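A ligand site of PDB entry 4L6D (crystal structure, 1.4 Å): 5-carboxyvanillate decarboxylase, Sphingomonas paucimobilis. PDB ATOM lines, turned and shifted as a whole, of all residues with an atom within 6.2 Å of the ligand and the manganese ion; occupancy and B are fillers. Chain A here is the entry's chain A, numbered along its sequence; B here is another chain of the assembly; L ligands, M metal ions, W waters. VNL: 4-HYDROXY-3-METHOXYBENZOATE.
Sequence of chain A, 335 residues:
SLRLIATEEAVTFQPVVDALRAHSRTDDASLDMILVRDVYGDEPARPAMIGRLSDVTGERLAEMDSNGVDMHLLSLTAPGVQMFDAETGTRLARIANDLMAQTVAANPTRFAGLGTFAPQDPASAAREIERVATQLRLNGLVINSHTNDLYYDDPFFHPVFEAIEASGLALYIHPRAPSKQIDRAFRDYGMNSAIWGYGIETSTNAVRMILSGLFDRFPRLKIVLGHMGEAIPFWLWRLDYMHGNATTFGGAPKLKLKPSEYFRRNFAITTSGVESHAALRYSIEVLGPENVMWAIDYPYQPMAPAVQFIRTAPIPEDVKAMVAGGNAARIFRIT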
ATOM      1  N   GLU A   8     -32.872  25.148 -14.399  1.00  0.00           N
ATOM      2  CA  GLU A   8     -31.785  25.276 -13.421  1.00  0.00           C
ATOM      3  C   GLU A   8     -30.768  26.316 -13.880  1.00  0.00           C
ATOM      4  O   GLU A   8     -29.577  26.022 -14.025  1.00  0.00           O
ATOM      5  CB  GLU A   8     -31.066  23.945 -13.151  1.00  0.00           C
ATOM      6  CG  GLU A   8     -30.340  23.952 -11.788  1.00  0.00           C
ATOM      7  CD  GLU A   8     -29.456  22.732 -11.578  1.00  0.00           C
ATOM      8  OE1 GLU A   8     -30.004  21.603 -11.487  1.00  0.00           O
ATOM      9  OE2 GLU A   8     -28.217  22.887 -11.496  1.00  0.00           O
ATOM     10  N   GLU A   9     -31.245  27.540 -14.090  1.00  0.00           N
ATOM     11  CA  GLU A   9     -30.464  28.521 -14.801  1.00  0.00           C
ATOM     12  C   GLU A   9     -29.996  29.571 -13.824  1.00  0.00           C
ATOM     13  O   GLU A   9     -30.783  30.353 -13.303  1.00  0.00           O
ATOM     14  CB  GLU A   9     -31.280  29.097 -15.971  1.00  0.00           C
ATOM     15  CG  GLU A   9     -31.990  27.986 -16.769  1.00  0.00           C
ATOM     16  CD  GLU A   9     -31.066  26.814 -17.063  1.00  0.00           C
ATOM     17  OE1 GLU A   9     -31.465  25.637 -16.853  1.00  0.00           O
ATOM     18  OE2 GLU A   9     -29.918  27.073 -17.495  1.00  0.00           O
ATOM     19  N   ALA A  10     -28.694  29.558 -13.565  1.00  0.00           N
ATOM     20  CA  ALA A  10     -28.089  30.355 -12.509  1.00  0.00           C
ATOM     21  C   ALA A  10     -27.951  31.817 -12.887  1.00  0.00           C
ATOM     22  O   ALA A  10     -27.695  32.158 -14.053  1.00  0.00           O
ATOM     23  CB  ALA A  10     -26.720  29.783 -12.164  1.00  0.00           C
ATOM     24  N   LEU A  35     -14.875  26.800  -5.067  1.00  0.00           N
ATOM     25  CA  LEU A  35     -15.692  27.552  -6.017  1.00  0.00           C
ATOM     26  C   LEU A  35     -15.618  29.055  -5.744  1.00  0.00           C
ATOM     27  O   LEU A  35     -15.431  29.855  -6.671  1.00  0.00           O
ATOM     28  CB  LEU A  35     -17.158  27.116  -5.908  1.00  0.00           C
ATOM     29  CG  LEU A  35     -18.191  28.016  -6.589  1.00  0.00           C
ATOM     30  CD1 LEU A  35     -18.087  27.864  -8.086  1.00  0.00           C
ATOM     31  CD2 LEU A  35     -19.589  27.682  -6.096  1.00  0.00           C
ATOM     32  N   ARG A  46     -11.478  31.533 -12.664  1.00  0.00           N
ATOM     33  CA  ARG A  46     -12.608  31.536 -13.608  1.00  0.00           C
ATOM     34  C   ARG A  46     -13.150  32.962 -13.706  1.00  0.00           C
ATOM     35  O   ARG A  46     -14.265  33.248 -13.252  1.00  0.00           O
ATOM     36  CB  ARG A  46     -13.697  30.548 -13.150  1.00  0.00           C
ATOM     37  CG  ARG A  46     -13.186  29.097 -13.019  1.00  0.00           C
ATOM     38  CD  ARG A  46     -14.163  28.133 -12.314  1.00  0.00           C
ATOM     39  NE  ARG A  46     -15.269  27.706 -13.186  1.00  0.00           N
ATOM     40  CZ  ARG A  46     -16.247  26.891 -12.810  1.00  0.00           C
ATOM     41  NH1 ARG A  46     -16.275  26.406 -11.573  1.00  0.00           N
ATOM     42  NH2 ARG A  46     -17.194  26.548 -13.680  1.00  0.00           N
ATOM     43  N   MET A  49     -16.789  34.242 -15.143  1.00  0.00           N
ATOM     44  CA  MET A  49     -18.036  33.691 -14.633  1.00  0.00           C
ATOM     45  C   MET A  49     -18.973  34.712 -13.970  1.00  0.00           C
ATOM     46  O   MET A  49     -20.185  34.629 -14.156  1.00  0.00           O
ATOM     47  CB  MET A  49     -17.758  32.509 -13.718  1.00  0.00           C
ATOM     48  CG  MET A  49     -18.999  31.723 -13.337  1.00  0.00           C
ATOM     49  SD  MET A  49     -19.882  31.013 -14.751  1.00  0.00           S
ATOM     50  CE  MET A  49     -18.913  29.559 -15.112  1.00  0.00           C
ATOM     51  N   THR A  77     -27.327  31.668  -7.857  1.00  0.00           N
ATOM     52  CA  THR A  77     -26.369  30.581  -8.006  1.00  0.00           C
ATOM     53  C   THR A  77     -25.850  30.106  -6.653  1.00  0.00           C
ATOM     54  O   THR A  77     -25.756  30.891  -5.714  1.00  0.00           O
ATOM     55  CB  THR A  77     -25.199  31.037  -8.910  1.00  0.00           C
ATOM     56  OG1 THR A  77     -24.376  29.911  -9.234  1.00  0.00           O
ATOM     57  CG2 THR A  77     -24.371  32.140  -8.256  1.00  0.00           C
ATOM     58  N   ALA A  78     -25.554  28.818  -6.555  1.00  0.00           N
ATOM     59  CA  ALA A  78     -24.929  28.283  -5.352  1.00  0.00           C
ATOM     60  C   ALA A  78     -23.622  29.053  -5.103  1.00  0.00           C
ATOM     61  O   ALA A  78     -22.921  29.436  -6.042  1.00  0.00           O
ATOM     62  CB  ALA A  78     -24.645  26.801  -5.534  1.00  0.00           C
ATOM     63  N   PRO A  79     -23.271  29.272  -3.821  1.00  0.00           N
ATOM     64  CA  PRO A  79     -23.918  28.797  -2.589  1.00  0.00           C
ATOM     65  C   PRO A  79     -25.014  29.714  -2.057  1.00  0.00           C
ATOM     66  O   PRO A  79     -25.338  29.658  -0.864  1.00  0.00           O
ATOM     67  CB  PRO A  79     -22.753  28.759  -1.604  1.00  0.00           C
ATOM     68  CG  PRO A  79     -21.925  29.949  -2.016  1.00  0.00           C
ATOM     69  CD  PRO A  79     -22.020  29.999  -3.529  1.00  0.00           C
ATOM     70  N   HIS A 174     -30.809  22.660  -5.000  1.00  0.00           N
ATOM     71  CA  HIS A 174     -29.646  22.692  -5.882  1.00  0.00           C
ATOM     72  C   HIS A 174     -28.433  22.200  -5.096  1.00  0.00           C
ATOM     73  O   HIS A 174     -28.433  22.272  -3.867  1.00  0.00           O
ATOM     74  CB  HIS A 174     -29.457  24.139  -6.330  1.00  0.00           C
ATOM     75  CG  HIS A 174     -28.412  24.330  -7.378  1.00  0.00           C
ATOM     76  ND1 HIS A 174     -27.067  24.448  -7.077  1.00  0.00           N
ATOM     77  CD2 HIS A 174     -28.502  24.425  -8.723  1.00  0.00           C
ATOM     78  CE1 HIS A 174     -26.377  24.606  -8.194  1.00  0.00           C
ATOM     79  NE2 HIS A 174     -27.226  24.588  -9.203  1.00  0.00           N
ATOM     80  N   PRO A 175     -27.391  21.705  -5.778  1.00  0.00           N
ATOM     81  CA  PRO A 175     -26.197  21.325  -4.997  1.00  0.00           C
ATOM     82  C   PRO A 175     -25.399  22.506  -4.416  1.00  0.00           C
ATOM     83  O   PRO A 175     -25.555  23.676  -4.772  1.00  0.00           O
ATOM     84  CB  PRO A 175     -25.320  20.592  -6.034  1.00  0.00           C
ATOM     85  CG  PRO A 175     -26.287  20.150  -7.099  1.00  0.00           C
ATOM     86  CD  PRO A 175     -27.334  21.212  -7.167  1.00  0.00           C
ATOM     87  N   SER A 193     -16.751  19.421  -6.770  1.00  0.00           N
ATOM     88  CA  SER A 193     -17.673  20.131  -7.634  1.00  0.00           C
ATOM     89  C   SER A 193     -18.671  19.185  -8.312  1.00  0.00           C
ATOM     90  O   SER A 193     -19.005  18.105  -7.788  1.00  0.00           O
ATOM     91  CB  SER A 193     -16.836  20.927  -8.667  1.00  0.00           C
ATOM     92  OG  SER A 193     -17.625  21.805  -9.453  1.00  0.00           O
ATOM     93  N   ALA A 194     -19.136  19.583  -9.493  1.00  0.00           N
ATOM     94  CA  ALA A 194     -20.175  18.872 -10.222  1.00  0.00           C
ATOM     95  C   ALA A 194     -19.814  17.442 -10.629  1.00  0.00           C
ATOM     96  O   ALA A 194     -20.710  16.596 -10.764  1.00  0.00           O
ATOM     97  CB  ALA A 194     -20.588  19.686 -11.445  1.00  0.00           C
ATOM     98  N   TYR A 198     -21.021  17.272  -5.752  1.00  0.00           N
ATOM     99  CA  TYR A 198     -22.351  17.887  -5.780  1.00  0.00           C
ATOM    100  C   TYR A 198     -23.472  16.850  -5.660  1.00  0.00           C
ATOM    101  O   TYR A 198     -24.434  17.046  -4.914  1.00  0.00           O
ATOM    102  CB  TYR A 198     -22.538  18.707  -7.069  1.00  0.00           C
ATOM    103  CG  TYR A 198     -21.950  20.101  -7.004  1.00  0.00           C
ATOM    104  CD1 TYR A 198     -21.097  20.487  -5.964  1.00  0.00           C
ATOM    105  CD2 TYR A 198     -22.276  21.042  -7.976  1.00  0.00           C
ATOM    106  CE1 TYR A 198     -20.574  21.790  -5.913  1.00  0.00           C
ATOM    107  CE2 TYR A 198     -21.751  22.330  -7.944  1.00  0.00           C
ATOM    108  CZ  TYR A 198     -20.901  22.694  -6.902  1.00  0.00           C
ATOM    109  OH  TYR A 198     -20.412  23.984  -6.859  1.00  0.00           O
ATOM    110  N   HIS A 227     -29.854  17.307 -12.114  1.00  0.00           N
ATOM    111  CA  HIS A 227     -28.859  16.269 -12.406  1.00  0.00           C
ATOM    112  C   HIS A 227     -29.474  14.891 -12.351  1.00  0.00           C
ATOM    113  O   HIS A 227     -28.961  13.966 -11.706  1.00  0.00           O
ATOM    114  CB  HIS A 227     -27.648  16.465 -11.485  1.00  0.00           C
ATOM    115  CG  HIS A 227     -27.310  17.906 -11.356  1.00  0.00           C
ATOM    116  ND1 HIS A 227     -27.549  18.623 -10.205  1.00  0.00           N
ATOM    117  CD2 HIS A 227     -26.903  18.807 -12.284  1.00  0.00           C
ATOM    118  CE1 HIS A 227     -27.266  19.895 -10.417  1.00  0.00           C
ATOM    119  NE2 HIS A 227     -26.872  20.032 -11.675  1.00  0.00           N
ATOM    120  N   SER A 272     -30.686  18.719 -15.790  1.00  0.00           N
ATOM    121  CA  SER A 272     -29.485  19.558 -15.813  1.00  0.00           C
ATOM    122  C   SER A 272     -28.217  18.720 -15.742  1.00  0.00           C
ATOM    123  O   SER A 272     -28.086  17.849 -14.880  1.00  0.00           O
ATOM    124  CB  SER A 272     -29.495  20.544 -14.651  1.00  0.00           C
ATOM    125  OG  SER A 272     -29.728  19.858 -13.428  1.00  0.00           O
ATOM    126  N   ASP A 297     -28.541  24.172 -16.942  1.00  0.00           N
ATOM    127  CA  ASP A 297     -27.465  24.525 -16.015  1.00  0.00           C
ATOM    128  C   ASP A 297     -26.557  25.635 -16.595  1.00  0.00           C
ATOM    129  O   ASP A 297     -25.352  25.640 -16.365  1.00  0.00           O
ATOM    130  CB  ASP A 297     -26.631  23.307 -15.594  1.00  0.00           C
ATOM    131  CG  ASP A 297     -26.412  23.242 -14.093  1.00  0.00           C
ATOM    132  OD1 ASP A 297     -26.540  24.278 -13.422  1.00  0.00           O
ATOM    133  OD2 ASP A 297     -26.111  22.138 -13.594  1.00  0.00           O
ATOM    134  N   TYR A 298     -27.152  26.562 -17.338  1.00  0.00           N
ATOM    135  CA  TYR A 298     -26.449  27.748 -17.837  1.00  0.00           C
ATOM    136  C   TYR A 298     -26.166  28.663 -16.628  1.00  0.00           C
ATOM    137  O   TYR A 298     -26.973  28.735 -15.720  1.00  0.00           O
ATOM    138  CB  TYR A 298     -27.333  28.456 -18.862  1.00  0.00           C
ATOM    139  CG  TYR A 298     -26.694  29.670 -19.471  1.00  0.00           C
ATOM    140  CD1 TYR A 298     -25.897  29.564 -20.607  1.00  0.00           C
ATOM    141  CD2 TYR A 298     -26.857  30.932 -18.899  1.00  0.00           C
ATOM    142  CE1 TYR A 298     -25.297  30.673 -21.159  1.00  0.00           C
ATOM    143  CE2 TYR A 298     -26.257  32.041 -19.452  1.00  0.00           C
ATOM    144  CZ  TYR A 298     -25.477  31.911 -20.586  1.00  0.00           C
ATOM    145  OH  TYR A 298     -24.867  33.000 -21.148  1.00  0.00           O
ATOM    146  N   TYR A 300     -23.028  27.503 -16.498  1.00  0.00           N
ATOM    147  CA  TYR A 300     -22.019  26.494 -16.231  1.00  0.00           C
ATOM    148  C   TYR A 300     -21.926  25.452 -17.353  1.00  0.00           C
ATOM    149  O   TYR A 300     -20.901  24.785 -17.495  1.00  0.00           O
ATOM    150  CB  TYR A 300     -22.282  25.852 -14.870  1.00  0.00           C
ATOM    151  CG  TYR A 300     -22.240  26.860 -13.730  1.00  0.00           C
ATOM    152  CD1 TYR A 300     -21.022  27.352 -13.255  1.00  0.00           C
ATOM    153  CD2 TYR A 300     -23.410  27.330 -13.134  1.00  0.00           C
ATOM    154  CE1 TYR A 300     -20.971  28.285 -12.222  1.00  0.00           C
ATOM    155  CE2 TYR A 300     -23.364  28.254 -12.090  1.00  0.00           C
ATOM    156  CZ  TYR A 300     -22.145  28.731 -11.644  1.00  0.00           C
ATOM    157  OH  TYR A 300     -22.091  29.650 -10.610  1.00  0.00           O
ATOM    158  N   GLN A 301     -23.006  25.321 -18.120  1.00  0.00           N
ATOM    159  CA  GLN A 301     -23.024  24.501 -19.330  1.00  0.00           C
ATOM    160  C   GLN A 301     -23.633  25.300 -20.467  1.00  0.00           C
ATOM    161  O   GLN A 301     -24.411  26.229 -20.224  1.00  0.00           O
ATOM    162  CB  GLN A 301     -23.807  23.217 -19.105  1.00  0.00           C
ATOM    163  CG  GLN A 301     -23.167  22.340 -18.055  1.00  0.00           C
ATOM    164  CD  GLN A 301     -23.558  20.876 -18.171  1.00  0.00           C
ATOM    165  OE1 GLN A 301     -23.440  20.143 -17.216  1.00  0.00           O
ATOM    166  NE2 GLN A 301     -23.971  20.450 -19.361  1.00  0.00           N
ATOM    167  N   ARG B 238     -22.235  12.673 -16.907  1.00  0.00           N
ATOM    168  CA  ARG B 238     -21.799  13.796 -16.093  1.00  0.00           C
ATOM    169  C   ARG B 238     -20.331  13.674 -15.693  1.00  0.00           C
ATOM    170  O   ARG B 238     -19.604  14.660 -15.641  1.00  0.00           O
ATOM    171  CB  ARG B 238     -22.702  13.910 -14.865  1.00  0.00           C
ATOM    172  CG  ARG B 238     -22.415  15.085 -13.930  1.00  0.00           C
ATOM    173  CD  ARG B 238     -23.743  15.472 -13.305  1.00  0.00           C
ATOM    174  NE  ARG B 238     -23.695  16.402 -12.172  1.00  0.00           N
ATOM    175  CZ  ARG B 238     -23.652  17.717 -12.280  1.00  0.00           C
ATOM    176  NH1 ARG B 238     -23.565  18.286 -13.483  1.00  0.00           N
ATOM    177  NH2 ARG B 238     -23.677  18.475 -11.186  1.00  0.00           N
ATOM    178  N   MET B 242     -17.886  16.741 -16.932  1.00  0.00           N
ATOM    179  CA  MET B 242     -17.214  17.595 -15.960  1.00  0.00           C
ATOM    180  C   MET B 242     -15.723  17.328 -15.824  1.00  0.00           C
ATOM    181  O   MET B 242     -15.028  18.039 -15.096  1.00  0.00           O
ATOM    182  CB  MET B 242     -17.916  17.476 -14.604  1.00  0.00           C
ATOM    183  CG  MET B 242     -19.239  18.239 -14.550  1.00  0.00           C
ATOM    184  SD  MET B 242     -18.996  19.986 -14.895  1.00  0.00           S
ATOM    185  CE  MET B 242     -20.712  20.576 -14.992  1.00  0.00           C
ATOM    186  N   ASN B 245     -13.268  20.298 -16.416  1.00  0.00           N
ATOM    187  CA  ASN B 245     -13.156  21.230 -15.295  1.00  0.00           C
ATOM    188  C   ASN B 245     -12.242  20.651 -14.226  1.00  0.00           C
ATOM    189  O   ASN B 245     -11.480  21.369 -13.581  1.00  0.00           O
ATOM    190  CB  ASN B 245     -14.520  21.531 -14.685  1.00  0.00           C
ATOM    191  CG  ASN B 245     -15.357  22.463 -15.542  1.00  0.00           C
ATOM    192  OD1 ASN B 245     -14.842  23.155 -16.432  1.00  0.00           O
ATOM    193  ND2 ASN B 245     -16.659  22.501 -15.261  1.00  0.00           N
HETATM  194  C1  VNL L   1     -20.814  24.571 -11.466  1.00  0.00           C
HETATM  195  CO1 VNL L   1     -21.741  23.862 -12.249  1.00  0.00           C
HETATM  196  CO2 VNL L   1     -21.241  25.402 -10.416  1.00  0.00           C
HETATM  197  CM1 VNL L   1     -23.116  23.986 -12.000  1.00  0.00           C
HETATM  198  CM2 VNL L   1     -22.601  25.530 -10.148  1.00  0.00           C
HETATM  199  OM  VNL L   1     -23.102  26.325  -9.144  1.00  0.00           O
HETATM  200  CZ  VNL L   1     -23.577  24.804 -10.968  1.00  0.00           C
HETATM  201  CC  VNL L   1     -19.349  24.451 -11.777  1.00  0.00           C
HETATM  202  CV  VNL L   1     -22.220  27.059  -8.282  1.00  0.00           C
HETATM  203  O1  VNL L   1     -18.960  23.963 -12.874  1.00  0.00           O
HETATM  204  O2  VNL L   1     -18.524  24.915 -10.950  1.00  0.00           O
HETATM  205  O3  VNL L   1     -24.871  25.230 -10.867  1.00  0.00           O
HETATM  206 MN    MN M   1     -26.700  24.448 -11.333  1.00  0.00          MN
HETATM  207  O   HOH W   1     -18.239  24.130  -8.484  1.00  0.00           O
HETATM  208  O   HOH W   2     -25.694  27.509  -9.350  1.00  0.00           O
HETATM  209  O   HOH W   3     -24.084  21.297 -11.238  1.00  0.00           O
HETATM  210  O   HOH W   4     -27.772  26.314 -11.791  1.00  0.00           O
HETATM  211  O   HOH W   5     -18.986  24.125 -15.626  1.00  0.00           O
HETATM  212  O   HOH W   6     -16.838  22.438 -12.129  1.00  0.00           O
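An oxygen (O2) of the ligand is in salt-bridge range of the guanidinium group (NH1) of Arg 46 (2.8 Å).
Water W1 lies within hydrogen-bond range of OG of Ser 193 (2.6 Å), O2 of the ligand (2.6 Å) and OH of Tyr 198 (2.7 Å).
Water W6 lies within hydrogen-bond range of O1 of the ligand (2.7 Å), OG of Ser 193 (2.9 Å) and ND2 of Asn 245 of chain B (3.1 Å).
Water W5 lies within hydrogen-bond range of the backbone carbonyl oxygen (O) of Tyr 300 (2.8 Å), an oxygen (O1) of the ligand (2.8 Å) and the side-chain amide nitrogen (ND2) of Asn 245 of chain B (2.9 Å).
Water W2 lies within hydrogen-bond range of the side-chain hydroxyl of Thr 77 (2.7 Å), an oxygen (OM) of the ligand (2.9 Å) and the backbone NH of Ala 78 (3.1 Å).
Water W3 lies within hydrogen-bond range of the guanidinium group of Arg 238 of chain B (2.9 Å), a ring nitrogen (NE2) of His 227 (3.1 Å) and the side-chain carboxylate of Asp 297 (3.2 Å).
Within 4 Å of the manganese ion: Glu 8, His 174 and Asp 297.
The nearest printed residue that does not touch the manganese ion is His 227 (4.4 Å).
Merely in contact with the ligand: Leu 35 (3.5 Å), Thr 77 (3.7 Å), Ala 78 (3.3 Å), Ser 193 (3.6 Å), Tyr 198 (3.8 Å), Tyr 300 (3.3 Å) and Asn 245 of chain B (3.6 Å).
Of the 23 residues printed, 10 come within 4 Å of the ligand.
The nearest printed residue that does not touch the ligand is Glu 8 (4.1 Å).
O of Ser 193 sits at hydrogen-bond distance from N of Tyr 198, 3.0 Å away.
ND2 of Asn 245 of chain B lies within hydrogen-bond range of SD of Met 242 of chain B.
NE2 of His 227 sits close to OE2 of Glu 8, 3.2 Å away.
The side-chain carboxylate (OE1) of Glu 8 lies within hydrogen-bond range of the side-chain hydroxyl (OG) of Ser 272 (2.6 Å).
The side-chain carboxylate of Asp 297 lies within hydrogen-bond range of a ring nitrogen (NE2) of His 227 (2.9 Å).
N of Asp 297 sits at hydrogen-bond distance from OE2 of Glu 9 (3.3 Å).
OG1 of Thr 77 sits at hydrogen-bond distance from OH of Tyr 300.
An oxygen (O3) of the ligand is bound to the manganese ion (2.0 Å).
The side-chain carboxylate (OD1) of Asp 297 is bound to the manganese ion, 2.1 Å away.
The side-chain carboxylate (OE2) of Glu 8 binds the manganese ion (2.2 Å).
NE2 of His 174 is bound to the manganese ion.
Water W4 binds the manganese ion (2.2 Å).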
